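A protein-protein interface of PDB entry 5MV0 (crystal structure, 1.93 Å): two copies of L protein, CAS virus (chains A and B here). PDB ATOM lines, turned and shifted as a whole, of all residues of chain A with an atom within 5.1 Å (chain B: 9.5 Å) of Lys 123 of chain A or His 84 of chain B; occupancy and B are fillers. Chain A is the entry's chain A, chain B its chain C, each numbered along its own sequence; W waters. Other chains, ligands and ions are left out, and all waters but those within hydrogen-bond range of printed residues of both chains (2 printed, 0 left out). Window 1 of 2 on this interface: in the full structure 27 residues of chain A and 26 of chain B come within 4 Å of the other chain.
Of the 24 printed residues of chain B, 8 touch a printed residue of chain A. Printed residues of chain A that touch a printed residue of chain B: Gln 83, Lys 116, Ser 119, Asp 120, Leu 122 and Lys 123. Among the printed residues, no Asp or Glu carboxylate lies within 4 Å of a Lys or Arg side-chain nitrogen of the other chain.
Gln 83 of chain A touches Ser 119 of chain B, and with the chains exchanged Ser 119 of chain A touches Gln 83 of chain B. Gln 83 of chain A touches Leu 122 of chain B, and with the chains exchanged Leu 122 of chain A touches Gln 83 of chain B. Gln 83 of chain A touches Lys 123 of chain B, and with the chains exchanged Lys 123 of chain A touches Gln 83 of chain B. Positions printed for both chains: 83, 85, 86, 103, 119, 120, 122, 123, 124 and 125.
NZ of Lys 116 of chain A lies within hydrogen-bond range of ND1 of His 84 of chain B (3.3 Å). The backbone carbonyl oxygen (O) of Ser 119 of chain A is in hydrogen-bond range of the backbone NH (N) of His 84 of chain B (2.8 Å).
Water W2 bridges NZ of Lys 116 of chain A and NE2 of His 84 of chain B. Water W1 bridges O of Lys 123 of chain B (3.0 Å) and O of Lys 123 of chain A (3.3 Å).
Of the printed residues of chain B, Lys 123 of chain A touches Gln 83 and His 84. His 84 of chain B touches just these residues of chain A: Lys 116 (3.3 Å), Ser 119 (2.8 Å), Asp 120 (3.5 Å) and Lys 123 (3.3 Å). No residue of chain B comes within 4 Å of Ser 125 of chain A. Of the printed residues of chain A, Phe 82 of chain B touches Ser 119 and Leu 122. Of the printed residues of chain B, Lys 116 of chain A touches His 84. Of the printed residues of chain A, Ser 119 of chain B touches Gln 83. Printed residues of chain A within 4 Å of Gln 83 of chain B: Ser 119 (3.4 Å), Leu 122 (3.8 Å) and Lys 123 (3.8 Å). Of the printed residues of chain A, Asn 69 of chain B touches Ser 119 (3.7 Å). The nearest residue of chain B that does not touch Lys 123 of chain A is Ile 85 of chain B (5.5 Å).
Among the printed residues, pairs that only touch across the chains: Ser 119 of chain A with Phe 82 of chain B (3.1 Å), Lys 123 of chain A with His 84 of chain B (3.3 Å), Leu 122 of chain A with Thr 81 of chain B (3.3 Å), Ser 119 of chain A with Gln 83 of chain B (3.4 Å), Gln 83 of chain A with Ser 119 of chain B (3.5 Å), Asp 120 of chain A with His 84 of chain B (3.5 Å), Ser 119 of chain A with Asn 69 of chain B (3.7 Å), Gln 83 of chain A with Leu 122 of chain B (3.8 Å), Leu 122 of chain A with Gln 83 of chain B (3.8 Å), Lys 123 of chain A with Gln 83 of chain B (3.8 Å), Leu 122 of chain A with Phe 82 of chain B (3.9 Å), Gln 83 of chain A with Lys 123 of chain B (3.9 Å) and Ser 119 of chain A with Thr 81 of chain B (3.9 Å).
O of Lys 123 of chain A sits at hydrogen-bond distance from NE2 of Gln 83 of chain A (2.7 Å). The backbone carbonyl oxygen (O) of Lys 116 of chain A lies within hydrogen-bond range of the side-chain hydroxyl (OG) of Ser 119 of chain A. The side-chain hydroxyl (OG) of Ser 67 of chain B lies close to the backbone NH (N) of Asn 69 of chain B (3.4 Å). The backbone carbonyl oxygen of Phe 82 of chain B is in hydrogen-bond range of the side-chain amide nitrogen of Asn 69 of chain B (2.8 Å). The side-chain amide nitrogen of Gln 83 of chain B lies within hydrogen-bond range of the backbone carbonyl oxygen of Ser 125 of chain B (3.0 Å). The side-chain hydroxyl of Ser 125 of chain B is in hydrogen-bond range of the backbone carbonyl oxygen of Leu 122 of chain B (2.8 Å).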
ATOM      1  N   GLN A  83       8.420 -14.125  -7.092  1.00  0.00           N
ATOM      2  CA  GLN A  83       9.044 -14.214  -5.783  1.00  0.00           C
ATOM      3  C   GLN A  83      10.514 -14.599  -5.922  1.00  0.00           C
ATOM      4  O   GLN A  83      10.896 -15.363  -6.819  1.00  0.00           O
ATOM      5  CB  GLN A  83       8.309 -15.255  -4.928  1.00  0.00           C
ATOM      6  CG  GLN A  83       8.215 -16.635  -5.579  1.00  0.00           C
ATOM      7  CD  GLN A  83       6.891 -16.883  -6.284  1.00  0.00           C
ATOM      8  OE1 GLN A  83       6.416 -16.049  -7.056  1.00  0.00           O
ATOM      9  NE2 GLN A  83       6.281 -18.025  -6.010  1.00  0.00           N
ATOM     10  N   ILE A  85      13.470 -16.763  -5.231  1.00  0.00           N
ATOM     11  CA  ILE A  85      13.752 -18.147  -4.850  1.00  0.00           C
ATOM     12  C   ILE A  85      15.122 -18.483  -5.410  1.00  0.00           C
ATOM     13  O   ILE A  85      15.442 -18.092  -6.533  1.00  0.00           O
ATOM     14  CB  ILE A  85      12.707 -19.134  -5.420  1.00  0.00           C
ATOM     15  CG1 ILE A  85      11.291 -18.844  -4.904  1.00  0.00           C
ATOM     16  CG2 ILE A  85      13.140 -20.624  -5.211  1.00  0.00           C
ATOM     17  CD1 ILE A  85      10.210 -19.704  -5.604  1.00  0.00           C
ATOM     18  N   VAL A  86      15.929 -19.217  -4.655  1.00  0.00           N
ATOM     19  CA  VAL A  86      17.168 -19.786  -5.170  1.00  0.00           C
ATOM     20  C   VAL A  86      17.074 -21.305  -5.071  1.00  0.00           C
ATOM     21  O   VAL A  86      17.303 -21.874  -3.995  1.00  0.00           O
ATOM     22  CB  VAL A  86      18.401 -19.249  -4.430  1.00  0.00           C
ATOM     23  CG1 VAL A  86      19.660 -19.879  -5.007  1.00  0.00           C
ATOM     24  CG2 VAL A  86      18.491 -17.703  -4.523  1.00  0.00           C
ATOM     25  N   GLU A 103      14.534 -28.833  -5.036  1.00  0.00           N
ATOM     26  CA  GLU A 103      14.765 -28.480  -3.643  1.00  0.00           C
ATOM     27  C   GLU A 103      15.081 -29.768  -2.889  1.00  0.00           C
ATOM     28  O   GLU A 103      14.272 -30.704  -2.890  1.00  0.00           O
ATOM     29  CB  GLU A 103      13.530 -27.793  -3.045  1.00  0.00           C
ATOM     30  CG  GLU A 103      13.107 -26.527  -3.787  1.00  0.00           C
ATOM     31  CD  GLU A 103      14.043 -25.348  -3.496  1.00  0.00           C
ATOM     32  OE1 GLU A 103      13.845 -24.265  -4.077  1.00  0.00           O
ATOM     33  OE2 GLU A 103      14.983 -25.499  -2.686  1.00  0.00           O
ATOM     34  N   LYS A 116       8.878 -30.055   5.744  1.00  0.00           N
ATOM     35  CA  LYS A 116       9.912 -29.374   4.967  1.00  0.00           C
ATOM     36  C   LYS A 116       9.570 -29.399   3.485  1.00  0.00           C
ATOM     37  O   LYS A 116       9.710 -28.385   2.786  1.00  0.00           O
ATOM     38  CB  LYS A 116      11.273 -30.035   5.233  1.00  0.00           C
ATOM     39  CG  LYS A 116      12.469 -29.444   4.462  1.00  0.00           C
ATOM     40  CD  LYS A 116      12.573 -27.916   4.617  1.00  0.00           C
ATOM     41  CE  LYS A 116      13.838 -27.395   3.912  1.00  0.00           C
ATOM     42  NZ  LYS A 116      13.851 -25.912   3.762  1.00  0.00           N
ATOM     43  N   SER A 119       6.996 -26.760   2.941  1.00  0.00           N
ATOM     44  CA  SER A 119       7.512 -25.393   2.980  1.00  0.00           C
ATOM     45  C   SER A 119       8.308 -25.058   1.723  1.00  0.00           C
ATOM     46  O   SER A 119       8.260 -23.920   1.248  1.00  0.00           O
ATOM     47  CB  SER A 119       8.379 -25.174   4.227  1.00  0.00           C
ATOM     48  OG  SER A 119       9.603 -25.895   4.136  1.00  0.00           O
ATOM     49  N   ASP A 120       9.032 -26.039   1.162  1.00  0.00           N
ATOM     50  CA  ASP A 120       9.773 -25.800  -0.076  1.00  0.00           C
ATOM     51  C   ASP A 120       8.834 -25.689  -1.283  1.00  0.00           C
ATOM     52  O   ASP A 120       9.029 -24.820  -2.138  1.00  0.00           O
ATOM     53  CB  ASP A 120      10.813 -26.906  -0.307  1.00  0.00           C
ATOM     54  CG  ASP A 120      12.058 -26.767   0.606  1.00  0.00           C
ATOM     55  OD1 ASP A 120      12.205 -25.739   1.297  1.00  0.00           O
ATOM     56  OD2 ASP A 120      12.912 -27.680   0.609  1.00  0.00           O
ATOM     57  N   LYS A 121       7.830 -26.572  -1.391  1.00  0.00           N
ATOM     58  CA  LYS A 121       6.866 -26.459  -2.486  1.00  0.00           C
ATOM     59  C   LYS A 121       6.130 -25.127  -2.444  1.00  0.00           C
ATOM     60  O   LYS A 121       5.875 -24.514  -3.491  1.00  0.00           O
ATOM     61  CB  LYS A 121       5.833 -27.595  -2.441  1.00  0.00           C
ATOM     62  CG  LYS A 121       6.335 -28.970  -2.836  1.00  0.00           C
ATOM     63  CD  LYS A 121       5.156 -29.959  -2.894  1.00  0.00           C
ATOM     64  CE  LYS A 121       5.613 -31.397  -3.089  1.00  0.00           C
ATOM     65  NZ  LYS A 121       6.231 -31.621  -4.432  1.00  0.00           N
ATOM     66  N   LEU A 122       5.756 -24.678  -1.239  1.00  0.00           N
ATOM     67  CA  LEU A 122       4.925 -23.481  -1.118  1.00  0.00           C
ATOM     68  C   LEU A 122       5.634 -22.241  -1.635  1.00  0.00           C
ATOM     69  O   LEU A 122       4.966 -21.282  -2.036  1.00  0.00           O
ATOM     70  CB  LEU A 122       4.500 -23.263   0.338  1.00  0.00           C
ATOM     71  CG  LEU A 122       3.304 -24.079   0.864  1.00  0.00           C
ATOM     72  CD1 LEU A 122       3.142 -23.886   2.397  1.00  0.00           C
ATOM     73  CD2 LEU A 122       2.009 -23.704   0.117  1.00  0.00           C
ATOM     74  N   LYS A 123       6.979 -22.229  -1.629  1.00  0.00           N
ATOM     75  CA  LYS A 123       7.709 -21.098  -2.204  1.00  0.00           C
ATOM     76  C   LYS A 123       7.254 -20.791  -3.627  1.00  0.00           C
ATOM     77  O   LYS A 123       7.238 -19.625  -4.047  1.00  0.00           O
ATOM     78  CB  LYS A 123       9.221 -21.372  -2.248  1.00  0.00           C
ATOM     79  CG  LYS A 123       9.901 -21.676  -0.923  1.00  0.00           C
ATOM     80  CD  LYS A 123      11.423 -21.530  -1.039  1.00  0.00           C
ATOM     81  CE  LYS A 123      12.008 -22.543  -2.011  1.00  0.00           C
ATOM     82  NZ  LYS A 123      13.511 -22.486  -2.011  1.00  0.00           N
ATOM     83  N   TYR A 124       6.908 -21.824  -4.387  1.00  0.00           N
ATOM     84  CA  TYR A 124       6.691 -21.718  -5.823  1.00  0.00           C
ATOM     85  C   TYR A 124       5.244 -21.419  -6.218  1.00  0.00           C
ATOM     86  O   TYR A 124       4.910 -21.567  -7.397  1.00  0.00           O
ATOM     87  CB  TYR A 124       7.136 -23.008  -6.511  1.00  0.00           C
ATOM     88  CG  TYR A 124       8.635 -23.218  -6.469  1.00  0.00           C
ATOM     89  CD1 TYR A 124       9.458 -22.654  -7.432  1.00  0.00           C
ATOM     90  CD2 TYR A 124       9.219 -23.977  -5.468  1.00  0.00           C
ATOM     91  CE1 TYR A 124      10.838 -22.850  -7.406  1.00  0.00           C
ATOM     92  CE2 TYR A 124      10.607 -24.169  -5.428  1.00  0.00           C
ATOM     93  CZ  TYR A 124      11.402 -23.601  -6.403  1.00  0.00           C
ATOM     94  OH  TYR A 124      12.771 -23.777  -6.385  1.00  0.00           O
ATOM     95  N   SER A 125       4.394 -21.007  -5.279  1.00  0.00           N
ATOM     96  CA  SER A 125       2.983 -20.773  -5.587  1.00  0.00           C
ATOM     97  C   SER A 125       2.839 -19.828  -6.774  1.00  0.00           C
ATOM     98  O   SER A 125       3.519 -18.802  -6.848  1.00  0.00           O
ATOM     99  CB  SER A 125       2.271 -20.191  -4.364  1.00  0.00           C
ATOM    100  OG  SER A 125       2.373 -21.086  -3.262  1.00  0.00           O
ATOM    101  N   ASN B  62      20.287 -12.137  11.088  1.00  0.00           N
ATOM    102  CA  ASN B  62      19.957 -13.565  11.112  1.00  0.00           C
ATOM    103  C   ASN B  62      21.118 -14.439  10.605  1.00  0.00           C
ATOM    104  O   ASN B  62      21.001 -15.189   9.642  1.00  0.00           O
ATOM    105  CB  ASN B  62      18.690 -13.790  10.292  1.00  0.00           C
ATOM    106  CG  ASN B  62      18.137 -15.213  10.417  1.00  0.00           C
ATOM    107  OD1 ASN B  62      18.445 -15.945  11.369  1.00  0.00           O
ATOM    108  ND2 ASN B  62      17.307 -15.604   9.454  1.00  0.00           N
ATOM    109  N   LYS B  64      22.412 -17.028  12.005  1.00  0.00           N
ATOM    110  CA  LYS B  64      22.153 -18.452  12.167  1.00  0.00           C
ATOM    111  C   LYS B  64      21.147 -18.988  11.152  1.00  0.00           C
ATOM    112  O   LYS B  64      20.885 -20.195  11.141  1.00  0.00           O
ATOM    113  CB  LYS B  64      21.683 -18.740  13.589  1.00  0.00           C
ATOM    114  CG  LYS B  64      22.731 -18.452  14.636  1.00  0.00           C
ATOM    115  CD  LYS B  64      22.135 -18.657  16.010  1.00  0.00           C
ATOM    116  CE  LYS B  64      22.485 -17.519  16.955  1.00  0.00           C
ATOM    117  NZ  LYS B  64      21.923 -17.825  18.312  1.00  0.00           N
ATOM    118  N   GLU B  65      20.587 -18.113  10.318  1.00  0.00           N
ATOM    119  CA  GLU B  65      19.754 -18.488   9.171  1.00  0.00           C
ATOM    120  C   GLU B  65      18.526 -19.293   9.593  1.00  0.00           C
ATOM    121  O   GLU B  65      18.157 -20.297   8.984  1.00  0.00           O
ATOM    122  CB  GLU B  65      20.594 -19.220   8.125  1.00  0.00           C
ATOM    123  CG  GLU B  65      21.741 -18.325   7.627  1.00  0.00           C
ATOM    124  CD  GLU B  65      22.505 -18.913   6.455  1.00  0.00           C
ATOM    125  OE1 GLU B  65      23.324 -18.180   5.858  1.00  0.00           O
ATOM    126  OE2 GLU B  65      22.285 -20.095   6.127  1.00  0.00           O
ATOM    127  N   ILE B  66      17.860 -18.823  10.618  1.00  0.00           N
ATOM    128  CA  ILE B  66      16.618 -19.481  10.999  1.00  0.00           C
ATOM    129  C   ILE B  66      15.533 -19.083  10.009  1.00  0.00           C
ATOM    130  O   ILE B  66      15.558 -17.992   9.417  1.00  0.00           O
ATOM    131  CB  ILE B  66      16.219 -19.155  12.450  1.00  0.00           C
ATOM    132  CG1 ILE B  66      15.738 -17.714  12.592  1.00  0.00           C
ATOM    133  CG2 ILE B  66      17.391 -19.449  13.418  1.00  0.00           C
ATOM    134  CD1 ILE B  66      15.126 -17.450  13.967  1.00  0.00           C
ATOM    135  N   SER B  67      14.597 -19.998   9.783  1.00  0.00           N
ATOM    136  CA  SER B  67      13.573 -19.776   8.771  1.00  0.00           C
ATOM    137  C   SER B  67      12.405 -18.990   9.356  1.00  0.00           C
ATOM    138  O   SER B  67      12.274 -18.827  10.573  1.00  0.00           O
ATOM    139  CB  SER B  67      13.069 -21.106   8.225  1.00  0.00           C
ATOM    140  OG  SER B  67      12.330 -21.772   9.237  1.00  0.00           O
ATOM    141  N   LEU B  68      11.538 -18.514   8.463  1.00  0.00           N
ATOM    142  CA  LEU B  68      10.287 -17.904   8.905  1.00  0.00           C
ATOM    143  C   LEU B  68       9.480 -18.869   9.770  1.00  0.00           C
ATOM    144  O   LEU B  68       8.962 -18.485  10.825  1.00  0.00           O
ATOM    145  CB  LEU B  68       9.468 -17.466   7.689  1.00  0.00           C
ATOM    146  CG  LEU B  68       8.059 -16.974   8.015  1.00  0.00           C
ATOM    147  CD1 LEU B  68       8.152 -15.634   8.760  1.00  0.00           C
ATOM    148  CD2 LEU B  68       7.265 -16.874   6.725  1.00  0.00           C
ATOM    149  N   ASN B  69       9.364 -20.133   9.347  1.00  0.00           N
ATOM    150  CA  ASN B  69       8.621 -21.097  10.167  1.00  0.00           C
ATOM    151  C   ASN B  69       9.208 -21.201  11.569  1.00  0.00           C
ATOM    152  O   ASN B  69       8.467 -21.285  12.554  1.00  0.00           O
ATOM    153  CB  ASN B  69       8.595 -22.468   9.498  1.00  0.00           C
ATOM    154  CG  ASN B  69       7.505 -22.578   8.456  1.00  0.00           C
ATOM    155  OD1 ASN B  69       6.369 -22.203   8.711  1.00  0.00           O
ATOM    156  ND2 ASN B  69       7.853 -23.061   7.264  1.00  0.00           N
ATOM    157  N   MET B  70      10.541 -21.152  11.683  1.00  0.00           N
ATOM    158  CA  MET B  70      11.179 -21.176  12.996  1.00  0.00           C
ATOM    159  C   MET B  70      10.865 -19.923  13.797  1.00  0.00           C
ATOM    160  O   MET B  70      10.623 -20.002  15.005  1.00  0.00           O
ATOM    161  CB  MET B  70      12.698 -21.342  12.865  1.00  0.00           C
ATOM    162  CG  MET B  70      13.137 -22.754  12.463  1.00  0.00           C
ATOM    163  SD  MET B  70      14.804 -22.783  11.736  1.00  0.00           S
ATOM    164  CE  MET B  70      15.757 -22.543  13.189  1.00  0.00           C
ATOM    165  N   PRO B  80       0.093 -23.186  10.829  1.00  0.00           N
ATOM    166  CA  PRO B  80       0.249 -23.968   9.602  1.00  0.00           C
ATOM    167  C   PRO B  80       1.639 -23.760   9.021  1.00  0.00           C
ATOM    168  O   PRO B  80       2.279 -22.738   9.256  1.00  0.00           O
ATOM    169  CB  PRO B  80      -0.831 -23.396   8.684  1.00  0.00           C
ATOM    170  CG  PRO B  80      -0.912 -21.962   9.116  1.00  0.00           C
ATOM    171  CD  PRO B  80      -0.754 -21.998  10.611  1.00  0.00           C
ATOM    172  N   THR B  81       2.115 -24.751   8.274  1.00  0.00           N
ATOM    173  CA  THR B  81       3.434 -24.648   7.647  1.00  0.00           C
ATOM    174  C   THR B  81       3.434 -23.543   6.590  1.00  0.00           C
ATOM    175  O   THR B  81       2.613 -23.561   5.667  1.00  0.00           O
ATOM    176  CB  THR B  81       3.810 -25.986   7.024  1.00  0.00           C
ATOM    177  OG1 THR B  81       3.873 -26.982   8.054  1.00  0.00           O
ATOM    178  CG2 THR B  81       5.175 -25.896   6.323  1.00  0.00           C
ATOM    179  N   PHE B  82       4.352 -22.590   6.708  1.00  0.00           N
ATOM    180  CA  PHE B  82       4.507 -21.554   5.693  1.00  0.00           C
ATOM    181  C   PHE B  82       5.595 -21.919   4.685  1.00  0.00           C
ATOM    182  O   PHE B  82       6.373 -22.858   4.878  1.00  0.00           O
ATOM    183  CB  PHE B  82       4.844 -20.207   6.338  1.00  0.00           C
ATOM    184  CG  PHE B  82       3.756 -19.671   7.208  1.00  0.00           C
ATOM    185  CD1 PHE B  82       2.575 -19.189   6.655  1.00  0.00           C
ATOM    186  CD2 PHE B  82       3.897 -19.670   8.581  1.00  0.00           C
ATOM    187  CE1 PHE B  82       1.561 -18.698   7.470  1.00  0.00           C
ATOM    188  CE2 PHE B  82       2.885 -19.176   9.404  1.00  0.00           C
ATOM    189  CZ  PHE B  82       1.721 -18.702   8.852  1.00  0.00           C
ATOM    190  N   GLN B  83       5.641 -21.148   3.595  1.00  0.00           N
ATOM    191  CA  GLN B  83       6.737 -21.246   2.644  1.00  0.00           C
ATOM    192  C   GLN B  83       8.076 -21.072   3.360  1.00  0.00           C
ATOM    193  O   GLN B  83       8.192 -20.324   4.339  1.00  0.00           O
ATOM    194  CB  GLN B  83       6.589 -20.183   1.548  1.00  0.00           C
ATOM    195  CG  GLN B  83       6.534 -18.719   2.053  1.00  0.00           C
ATOM    196  CD  GLN B  83       5.095 -18.209   2.264  1.00  0.00           C
ATOM    197  OE1 GLN B  83       4.247 -18.914   2.810  1.00  0.00           O
ATOM    198  NE2 GLN B  83       4.822 -16.979   1.809  1.00  0.00           N
ATOM    199  N   HIS B  84       9.094 -21.786   2.872  1.00  0.00           N
ATOM    200  CA  HIS B  84      10.448 -21.614   3.390  1.00  0.00           C
ATOM    201  C   HIS B  84      10.973 -20.233   3.016  1.00  0.00           C
ATOM    202  O   HIS B  84      11.054 -19.898   1.833  1.00  0.00           O
ATOM    203  CB  HIS B  84      11.380 -22.690   2.832  1.00  0.00           C
ATOM    204  CG  HIS B  84      12.832 -22.424   3.119  1.00  0.00           C
ATOM    205  ND1 HIS B  84      13.419 -22.725   4.328  1.00  0.00           N
ATOM    206  CD2 HIS B  84      13.796 -21.830   2.371  1.00  0.00           C
ATOM    207  CE1 HIS B  84      14.692 -22.366   4.303  1.00  0.00           C
ATOM    208  NE2 HIS B  84      14.944 -21.816   3.128  1.00  0.00           N
ATOM    209  N   ILE B  85      11.357 -19.452   4.022  1.00  0.00           N
ATOM    210  CA  ILE B  85      11.993 -18.151   3.847  1.00  0.00           C
ATOM    211  C   ILE B  85      13.058 -18.026   4.927  1.00  0.00           C
ATOM    212  O   ILE B  85      12.820 -18.400   6.081  1.00  0.00           O
ATOM    213  CB  ILE B  85      10.979 -16.984   3.967  1.00  0.00           C
ATOM    214  CG1 ILE B  85       9.936 -17.013   2.833  1.00  0.00           C
ATOM    215  CG2 ILE B  85      11.695 -15.630   4.047  1.00  0.00           C
ATOM    216  CD1 ILE B  85       8.718 -16.062   3.101  1.00  0.00           C
ATOM    217  N   VAL B  86      14.219 -17.507   4.566  1.00  0.00           N
ATOM    218  CA  VAL B  86      15.246 -17.110   5.525  1.00  0.00           C
ATOM    219  C   VAL B  86      15.432 -15.609   5.423  1.00  0.00           C
ATOM    220  O   VAL B  86      16.091 -15.120   4.496  1.00  0.00           O
ATOM    221  CB  VAL B  86      16.568 -17.859   5.292  1.00  0.00           C
ATOM    222  CG1 VAL B  86      17.620 -17.445   6.327  1.00  0.00           C
ATOM    223  CG2 VAL B  86      16.346 -19.372   5.356  1.00  0.00           C
ATOM    224  N   PRO B  87      14.881 -14.828   6.344  1.00  0.00           N
ATOM    225  CA  PRO B  87      15.050 -13.372   6.288  1.00  0.00           C
ATOM    226  C   PRO B  87      16.462 -12.962   6.681  1.00  0.00           C
ATOM    227  O   PRO B  87      17.173 -13.694   7.372  1.00  0.00           O
ATOM    228  CB  PRO B  87      14.025 -12.845   7.302  1.00  0.00           C
ATOM    229  CG  PRO B  87      13.904 -13.931   8.286  1.00  0.00           C
ATOM    230  CD  PRO B  87      14.033 -15.238   7.482  1.00  0.00           C
ATOM    231  N   GLU B 103      14.381  -7.775   4.597  1.00  0.00           N
ATOM    232  CA  GLU B 103      15.055  -8.212   3.369  1.00  0.00           C
ATOM    233  C   GLU B 103      15.841  -7.021   2.829  1.00  0.00           C
ATOM    234  O   GLU B 103      15.250  -5.999   2.462  1.00  0.00           O
ATOM    235  CB  GLU B 103      14.060  -8.721   2.320  1.00  0.00           C
ATOM    236  CG  GLU B 103      13.221  -9.928   2.783  1.00  0.00           C
ATOM    237  CD  GLU B 103      14.023 -11.220   2.882  1.00  0.00           C
ATOM    238  OE1 GLU B 103      13.455 -12.232   3.342  1.00  0.00           O
ATOM    239  OE2 GLU B 103      15.209 -11.235   2.505  1.00  0.00           O
ATOM    240  N   SER B 119      10.363  -8.772  -5.824  1.00  0.00           N
ATOM    241  CA  SER B 119      10.576 -10.210  -5.678  1.00  0.00           C
ATOM    242  C   SER B 119      10.746 -10.593  -4.211  1.00  0.00           C
ATOM    243  O   SER B 119      10.264 -11.646  -3.780  1.00  0.00           O
ATOM    244  CB  SER B 119      11.797 -10.663  -6.490  1.00  0.00           C
ATOM    245  OG  SER B 119      12.982 -10.146  -5.931  1.00  0.00           O
ATOM    246  N   ASP B 120      11.408  -9.747  -3.424  1.00  0.00           N
ATOM    247  CA  ASP B 120      11.571 -10.050  -2.001  1.00  0.00           C
ATOM    248  C   ASP B 120      10.242  -9.956  -1.249  1.00  0.00           C
ATOM    249  O   ASP B 120       9.955 -10.783  -0.369  1.00  0.00           O
ATOM    250  CB  ASP B 120      12.611  -9.117  -1.376  1.00  0.00           C
ATOM    251  CG  ASP B 120      14.054  -9.531  -1.704  1.00  0.00           C
ATOM    252  OD1 ASP B 120      14.267 -10.580  -2.364  1.00  0.00           O
ATOM    253  OD2 ASP B 120      14.978  -8.816  -1.266  1.00  0.00           O
ATOM    254  N   LEU B 122       7.252 -10.443  -2.583  1.00  0.00           N
ATOM    255  CA  LEU B 122       6.373 -11.512  -3.044  1.00  0.00           C
ATOM    256  C   LEU B 122       6.630 -12.827  -2.326  1.00  0.00           C
ATOM    257  O   LEU B 122       5.730 -13.673  -2.286  1.00  0.00           O
ATOM    258  CB  LEU B 122       6.530 -11.706  -4.554  1.00  0.00           C
ATOM    259  CG  LEU B 122       5.755 -10.745  -5.457  1.00  0.00           C
ATOM    260  CD1 LEU B 122       6.115 -11.023  -6.906  1.00  0.00           C
ATOM    261  CD2 LEU B 122       4.252 -10.913  -5.232  1.00  0.00           C
ATOM    262  N   LYS B 123       7.838 -13.023  -1.770  1.00  0.00           N
ATOM    263  CA  LYS B 123       8.116 -14.247  -1.018  1.00  0.00           C
ATOM    264  C   LYS B 123       7.105 -14.462   0.095  1.00  0.00           C
ATOM    265  O   LYS B 123       6.768 -15.609   0.419  1.00  0.00           O
ATOM    266  CB  LYS B 123       9.504 -14.197  -0.369  1.00  0.00           C
ATOM    267  CG  LYS B 123      10.685 -14.107  -1.299  1.00  0.00           C
ATOM    268  CD  LYS B 123      12.002 -14.513  -0.561  1.00  0.00           C
ATOM    269  CE  LYS B 123      12.309 -13.619   0.622  1.00  0.00           C
ATOM    270  NZ  LYS B 123      13.653 -13.939   1.230  1.00  0.00           N
ATOM    271  N   TYR B 124       6.640 -13.375   0.711  1.00  0.00           N
ATOM    272  CA  TYR B 124       5.883 -13.433   1.952  1.00  0.00           C
ATOM    273  C   TYR B 124       4.377 -13.476   1.733  1.00  0.00           C
ATOM    274  O   TYR B 124       3.627 -13.214   2.680  1.00  0.00           O
ATOM    275  CB  TYR B 124       6.227 -12.234   2.839  1.00  0.00           C
ATOM    276  CG  TYR B 124       7.634 -12.244   3.389  1.00  0.00           C
ATOM    277  CD1 TYR B 124       7.911 -12.837   4.616  1.00  0.00           C
ATOM    278  CD2 TYR B 124       8.680 -11.665   2.684  1.00  0.00           C
ATOM    279  CE1 TYR B 124       9.192 -12.862   5.129  1.00  0.00           C
ATOM    280  CE2 TYR B 124       9.977 -11.685   3.190  1.00  0.00           C
ATOM    281  CZ  TYR B 124      10.220 -12.279   4.414  1.00  0.00           C
ATOM    282  OH  TYR B 124      11.490 -12.308   4.943  1.00  0.00           O
ATOM    283  N   SER B 125       3.917 -13.757   0.516  1.00  0.00           N
ATOM    284  CA  SER B 125       2.481 -13.716   0.244  1.00  0.00           C
ATOM    285  C   SER B 125       1.707 -14.570   1.248  1.00  0.00           C
ATOM    286  O   SER B 125       2.063 -15.727   1.512  1.00  0.00           O
ATOM    287  CB  SER B 125       2.202 -14.192  -1.180  1.00  0.00           C
ATOM    288  OG  SER B 125       2.909 -13.380  -2.100  1.00  0.00           O
ATOM    289  N   VAL B 127       1.481 -14.412   4.464  1.00  0.00           N
ATOM    290  CA  VAL B 127       1.995 -14.588   5.819  1.00  0.00           C
ATOM    291  C   VAL B 127       1.419 -13.541   6.762  1.00  0.00           C
ATOM    292  O   VAL B 127       0.946 -13.870   7.859  1.00  0.00           O
ATOM    293  CB  VAL B 127       3.532 -14.562   5.825  1.00  0.00           C
ATOM    294  CG1 VAL B 127       4.036 -14.549   7.264  1.00  0.00           C
ATOM    295  CG2 VAL B 127       4.071 -15.785   5.055  1.00  0.00           C
HETATM  296  O   HOH W   1       7.935 -17.685  -1.475  1.00  0.00           O
HETATM  297  O   HOH W   2      16.165 -25.019   2.741  1.00  0.00           O
